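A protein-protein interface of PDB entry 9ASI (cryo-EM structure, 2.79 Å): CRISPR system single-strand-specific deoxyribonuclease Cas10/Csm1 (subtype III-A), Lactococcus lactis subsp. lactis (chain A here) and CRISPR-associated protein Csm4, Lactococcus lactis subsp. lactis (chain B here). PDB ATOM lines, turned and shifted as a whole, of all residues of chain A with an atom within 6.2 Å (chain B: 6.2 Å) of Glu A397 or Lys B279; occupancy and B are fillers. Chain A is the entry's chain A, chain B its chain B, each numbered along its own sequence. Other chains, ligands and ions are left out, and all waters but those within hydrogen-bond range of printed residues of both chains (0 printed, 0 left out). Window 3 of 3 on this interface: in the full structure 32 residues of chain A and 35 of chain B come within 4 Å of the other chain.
OE2 of Glu A397 is in hydrogen-bond range of OH of Tyr B246, at 3.3 Å. The backbone carbonyl oxygen of Asn A398 sits at hydrogen-bond distance from the backbone NH of Lys B252. NE2 of Gln B254 lies within hydrogen-bond range of OE2 of Glu A397, 3.3 Å away. The backbone NH (N) of Lys B278 is in hydrogen-bond range of the side-chain carboxylate (OE2) of Glu A397, at 2.6 Å. N of Lys B279 sits close to OE1 of Glu A397, at 3.5 Å. O of Val B276 lies close to OE2 of Glu A397 (3.3 Å).
The side-chain hydroxyl (OH) of Tyr B246 sits at hydrogen-bond distance from the backbone NH (N) of Gly B280, at 3.5 Å. The backbone NH (N) of Gln B254 lies within hydrogen-bond range of the backbone carbonyl oxygen (O) of Val B276 (3.3 Å). The side-chain amide oxygen (OD1) of Asn A398 lies close to the backbone carbonyl oxygen (O) of Thr A396, at 2.8 Å.
Gln B254 touches Gly A395. Thr A396 touches Gln B254 (N to CG, 3.7 Å). Thr A396 touches Lys B279 (CG2 to NZ, 3.3 Å). Glu A397 touches Lys B252. OE2 of Glu A397 touches CA of Gly B277, 3.0 Å away. Asn A398 touches Val B251.
Of the printed residues of chain B, Thr A396 touches Gln B254 and Lys B279. Glu A397 touches just these residues of chain B: Tyr B246, Lys B252, Gln B254, Val B276, Gly B277, Lys B278 and Lys B279. Of the printed residues of chain B, Asn A398 touches Val B251 and Lys B252. Of the printed residues of chain A, Val B251 touches Asn A398. Of the printed residues of chain A, Lys B252 touches Glu A397 and Asn A398. Of the printed residues of chain A, Gly B277 touches Glu A397 (3.0 Å). Lys B279 touches two residues of chain A. Gly B280 touches none of the printed residues of chain A. Asn B281 touches none of the printed residues of chain A. The nearest residue of chain A that does not touch Lys B279 is Asn A398 (5.8 Å). The nearest printed residue of chain B that does not touch Asn A398 is Lys B253 (4.9 Å).
Of the 12 printed residues of chain B, 8 touch a printed residue of chain A. Printed residues of chain B that touch a printed residue of chain A: Tyr B246, Val B251, Lys B252, Gln B254, Val B276, Gly B277, Lys B278 and Lys B279. Printed residues of chain A that touch a printed residue of chain B: Gly A395, Thr A396, Glu A397 and Asn A398. Among the printed residues, no Asp or Glu carboxylate lies within 4 Å of a Lys or Arg side-chain nitrogen of the other chain.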
ATOM      1  N   GLY A 395       8.778  -3.716 -17.356  1.00  0.00           N
ATOM      2  CA  GLY A 395       7.874  -4.629 -18.019  1.00  0.00           C
ATOM      3  C   GLY A 395       6.620  -4.795 -17.194  1.00  0.00           C
ATOM      4  O   GLY A 395       6.691  -5.098 -15.999  1.00  0.00           O
ATOM      5  N   THR A 396       5.465  -4.586 -17.813  1.00  0.00           N
ATOM      6  CA  THR A 396       4.195  -4.600 -17.113  1.00  0.00           C
ATOM      7  C   THR A 396       3.213  -5.466 -17.883  1.00  0.00           C
ATOM      8  O   THR A 396       3.217  -5.478 -19.116  1.00  0.00           O
ATOM      9  CB  THR A 396       3.639  -3.179 -16.950  1.00  0.00           C
ATOM     10  OG1 THR A 396       4.672  -2.318 -16.456  1.00  0.00           O
ATOM     11  CG2 THR A 396       2.475  -3.161 -15.972  1.00  0.00           C
ATOM     12  N   GLU A 397       2.384  -6.200 -17.149  1.00  0.00           N
ATOM     13  CA  GLU A 397       1.349  -7.017 -17.763  1.00  0.00           C
ATOM     14  C   GLU A 397       0.181  -6.127 -18.161  1.00  0.00           C
ATOM     15  O   GLU A 397      -0.413  -5.458 -17.308  1.00  0.00           O
ATOM     16  CB  GLU A 397       0.888  -8.087 -16.783  1.00  0.00           C
ATOM     17  CG  GLU A 397       1.982  -9.004 -16.320  1.00  0.00           C
ATOM     18  CD  GLU A 397       1.512  -9.920 -15.222  1.00  0.00           C
ATOM     19  OE1 GLU A 397       0.342  -9.802 -14.804  1.00  0.00           O
ATOM     20  OE2 GLU A 397       2.324 -10.731 -14.744  1.00  0.00           O
ATOM     21  N   ASN A 398      -0.161  -6.125 -19.442  1.00  0.00           N
ATOM     22  CA  ASN A 398      -1.201  -5.252 -19.959  1.00  0.00           C
ATOM     23  C   ASN A 398      -2.325  -6.067 -20.585  1.00  0.00           C
ATOM     24  O   ASN A 398      -2.182  -7.255 -20.877  1.00  0.00           O
ATOM     25  CB  ASN A 398      -0.630  -4.269 -20.986  1.00  0.00           C
ATOM     26  CG  ASN A 398       0.344  -3.292 -20.372  1.00  0.00           C
ATOM     27  OD1 ASN A 398       1.526  -3.593 -20.222  1.00  0.00           O
ATOM     28  ND2 ASN A 398      -0.144  -2.112 -20.015  1.00  0.00           N
ATOM     29  N   ALA A 399      -3.458  -5.404 -20.782  1.00  0.00           N
ATOM     30  CA  ALA A 399      -4.577  -5.955 -21.533  1.00  0.00           C
ATOM     31  C   ALA A 399      -4.715  -5.344 -22.915  1.00  0.00           C
ATOM     32  O   ALA A 399      -5.023  -6.057 -23.872  1.00  0.00           O
ATOM     33  CB  ALA A 399      -5.885  -5.756 -20.760  1.00  0.00           C
ATOM     34  N   TYR B 246      -6.010 -18.095 -16.135  1.00  0.00           N
ATOM     35  CA  TYR B 246      -5.131 -16.990 -15.777  1.00  0.00           C
ATOM     36  C   TYR B 246      -5.883 -15.687 -15.982  1.00  0.00           C
ATOM     37  O   TYR B 246      -6.305 -15.386 -17.103  1.00  0.00           O
ATOM     38  CB  TYR B 246      -3.855 -17.009 -16.623  1.00  0.00           C
ATOM     39  CG  TYR B 246      -2.824 -15.955 -16.276  1.00  0.00           C
ATOM     40  CD1 TYR B 246      -1.833 -16.212 -15.343  1.00  0.00           C
ATOM     41  CD2 TYR B 246      -2.823 -14.721 -16.901  1.00  0.00           C
ATOM     42  CE1 TYR B 246      -0.884 -15.271 -15.030  1.00  0.00           C
ATOM     43  CE2 TYR B 246      -1.876 -13.770 -16.590  1.00  0.00           C
ATOM     44  CZ  TYR B 246      -0.911 -14.050 -15.654  1.00  0.00           C
ATOM     45  OH  TYR B 246       0.033 -13.099 -15.347  1.00  0.00           O
ATOM     46  N   ALA B 247      -6.075 -14.935 -14.901  1.00  0.00           N
ATOM     47  CA  ALA B 247      -6.511 -13.540 -14.946  1.00  0.00           C
ATOM     48  C   ALA B 247      -7.872 -13.341 -15.610  1.00  0.00           C
ATOM     49  O   ALA B 247      -8.197 -12.219 -16.008  1.00  0.00           O
ATOM     50  CB  ALA B 247      -5.465 -12.661 -15.640  1.00  0.00           C
ATOM     51  N   VAL B 251      -4.936 -11.257 -21.178  1.00  0.00           N
ATOM     52  CA  VAL B 251      -3.977 -10.292 -20.657  1.00  0.00           C
ATOM     53  C   VAL B 251      -2.591 -10.622 -21.196  1.00  0.00           C
ATOM     54  O   VAL B 251      -2.240 -11.795 -21.353  1.00  0.00           O
ATOM     55  CB  VAL B 251      -3.987 -10.278 -19.112  1.00  0.00           C
ATOM     56  CG1 VAL B 251      -3.605 -11.630 -18.572  1.00  0.00           C
ATOM     57  CG2 VAL B 251      -3.047  -9.217 -18.572  1.00  0.00           C
ATOM     58  N   LYS B 252      -1.820  -9.585 -21.512  1.00  0.00           N
ATOM     59  CA  LYS B 252      -0.445  -9.773 -21.943  1.00  0.00           C
ATOM     60  C   LYS B 252       0.454 -10.068 -20.747  1.00  0.00           C
ATOM     61  O   LYS B 252       0.051  -9.975 -19.585  1.00  0.00           O
ATOM     62  CB  LYS B 252       0.069  -8.543 -22.685  1.00  0.00           C
ATOM     63  CG  LYS B 252      -0.480  -8.374 -24.074  1.00  0.00           C
ATOM     64  CD  LYS B 252      -0.103  -7.026 -24.636  1.00  0.00           C
ATOM     65  CE  LYS B 252       1.338  -6.997 -25.082  1.00  0.00           C
ATOM     66  NZ  LYS B 252       1.520  -7.703 -26.365  1.00  0.00           N
ATOM     67  N   LYS B 253       1.698 -10.422 -21.047  1.00  0.00           N
ATOM     68  CA  LYS B 253       2.691 -10.729 -20.034  1.00  0.00           C
ATOM     69  C   LYS B 253       3.861  -9.760 -20.143  1.00  0.00           C
ATOM     70  O   LYS B 253       4.033  -9.069 -21.152  1.00  0.00           O
ATOM     71  CB  LYS B 253       3.178 -12.177 -20.158  1.00  0.00           C
ATOM     72  CG  LYS B 253       4.269 -12.388 -21.181  1.00  0.00           C
ATOM     73  CD  LYS B 253       4.509 -13.866 -21.413  1.00  0.00           C
ATOM     74  CE  LYS B 253       3.432 -14.463 -22.289  1.00  0.00           C
ATOM     75  NZ  LYS B 253       3.918 -15.638 -23.055  1.00  0.00           N
ATOM     76  N   GLN B 254       4.656  -9.707 -19.079  1.00  0.00           N
ATOM     77  CA  GLN B 254       5.793  -8.802 -19.023  1.00  0.00           C
ATOM     78  C   GLN B 254       6.801  -9.158 -20.104  1.00  0.00           C
ATOM     79  O   GLN B 254       7.346 -10.266 -20.112  1.00  0.00           O
ATOM     80  CB  GLN B 254       6.446  -8.876 -17.646  1.00  0.00           C
ATOM     81  CG  GLN B 254       5.731  -8.080 -16.581  1.00  0.00           C
ATOM     82  CD  GLN B 254       6.037  -8.572 -15.185  1.00  0.00           C
ATOM     83  OE1 GLN B 254       7.196  -8.778 -14.831  1.00  0.00           O
ATOM     84  NE2 GLN B 254       4.998  -8.756 -14.380  1.00  0.00           N
ATOM     85  N   VAL B 276       7.226 -14.265 -15.586  1.00  0.00           N
ATOM     86  CA  VAL B 276       6.718 -13.148 -16.373  1.00  0.00           C
ATOM     87  C   VAL B 276       5.229 -12.930 -16.174  1.00  0.00           C
ATOM     88  O   VAL B 276       4.684 -11.940 -16.673  1.00  0.00           O
ATOM     89  CB  VAL B 276       7.042 -13.324 -17.869  1.00  0.00           C
ATOM     90  CG1 VAL B 276       8.537 -13.352 -18.083  1.00  0.00           C
ATOM     91  CG2 VAL B 276       6.417 -14.601 -18.393  1.00  0.00           C
ATOM     92  N   GLY B 277       4.552 -13.827 -15.469  1.00  0.00           N
ATOM     93  CA  GLY B 277       3.190 -13.574 -15.058  1.00  0.00           C
ATOM     94  C   GLY B 277       3.045 -13.656 -13.555  1.00  0.00           C
ATOM     95  O   GLY B 277       3.115 -14.744 -12.980  1.00  0.00           O
ATOM     96  N   LYS B 278       2.821 -12.518 -12.908  1.00  0.00           N
ATOM     97  CA  LYS B 278       2.741 -12.445 -11.455  1.00  0.00           C
ATOM     98  C   LYS B 278       1.365 -12.065 -10.943  1.00  0.00           C
ATOM     99  O   LYS B 278       0.943 -12.562  -9.898  1.00  0.00           O
ATOM    100  CB  LYS B 278       3.768 -11.439 -10.921  1.00  0.00           C
ATOM    101  CG  LYS B 278       5.182 -11.683 -11.408  1.00  0.00           C
ATOM    102  CD  LYS B 278       6.054 -10.457 -11.221  1.00  0.00           C
ATOM    103  CE  LYS B 278       7.280 -10.517 -12.112  1.00  0.00           C
ATOM    104  NZ  LYS B 278       8.480 -10.999 -11.378  1.00  0.00           N
ATOM    105  N   LYS B 279       0.651 -11.193 -11.656  1.00  0.00           N
ATOM    106  CA  LYS B 279      -0.651 -10.742 -11.185  1.00  0.00           C
ATOM    107  C   LYS B 279      -1.735 -11.791 -11.389  1.00  0.00           C
ATOM    108  O   LYS B 279      -2.808 -11.676 -10.789  1.00  0.00           O
ATOM    109  CB  LYS B 279      -1.026  -9.435 -11.883  1.00  0.00           C
ATOM    110  CG  LYS B 279       0.006  -8.332 -11.690  1.00  0.00           C
ATOM    111  CD  LYS B 279      -0.032  -7.321 -12.821  1.00  0.00           C
ATOM    112  CE  LYS B 279       1.324  -6.660 -13.008  1.00  0.00           C
ATOM    113  NZ  LYS B 279       1.246  -5.453 -13.875  1.00  0.00           N
ATOM    114  N   GLY B 280      -1.482 -12.803 -12.214  1.00  0.00           N
ATOM    115  CA  GLY B 280      -2.404 -13.906 -12.365  1.00  0.00           C
ATOM    116  C   GLY B 280      -2.232 -14.940 -11.271  1.00  0.00           C
ATOM    117  O   GLY B 280      -1.408 -14.809 -10.367  1.00  0.00           O
ATOM    118  N   ASN B 281      -3.033 -15.999 -11.361  1.00  0.00           N
ATOM    119  CA  ASN B 281      -3.104 -16.989 -10.296  1.00  0.00           C
ATOM    120  C   ASN B 281      -2.306 -18.253 -10.591  1.00  0.00           C
ATOM    121  O   ASN B 281      -2.465 -19.248  -9.878  1.00  0.00           O
ATOM    122  CB  ASN B 281      -4.562 -17.341  -9.994  1.00  0.00           C
ATOM    123  CG  ASN B 281      -5.365 -17.609 -11.237  1.00  0.00           C
ATOM    124  OD1 ASN B 281      -5.012 -18.470 -12.036  1.00  0.00           O
ATOM    125  ND2 ASN B 281      -6.456 -16.873 -11.410  1.00  0.00           N
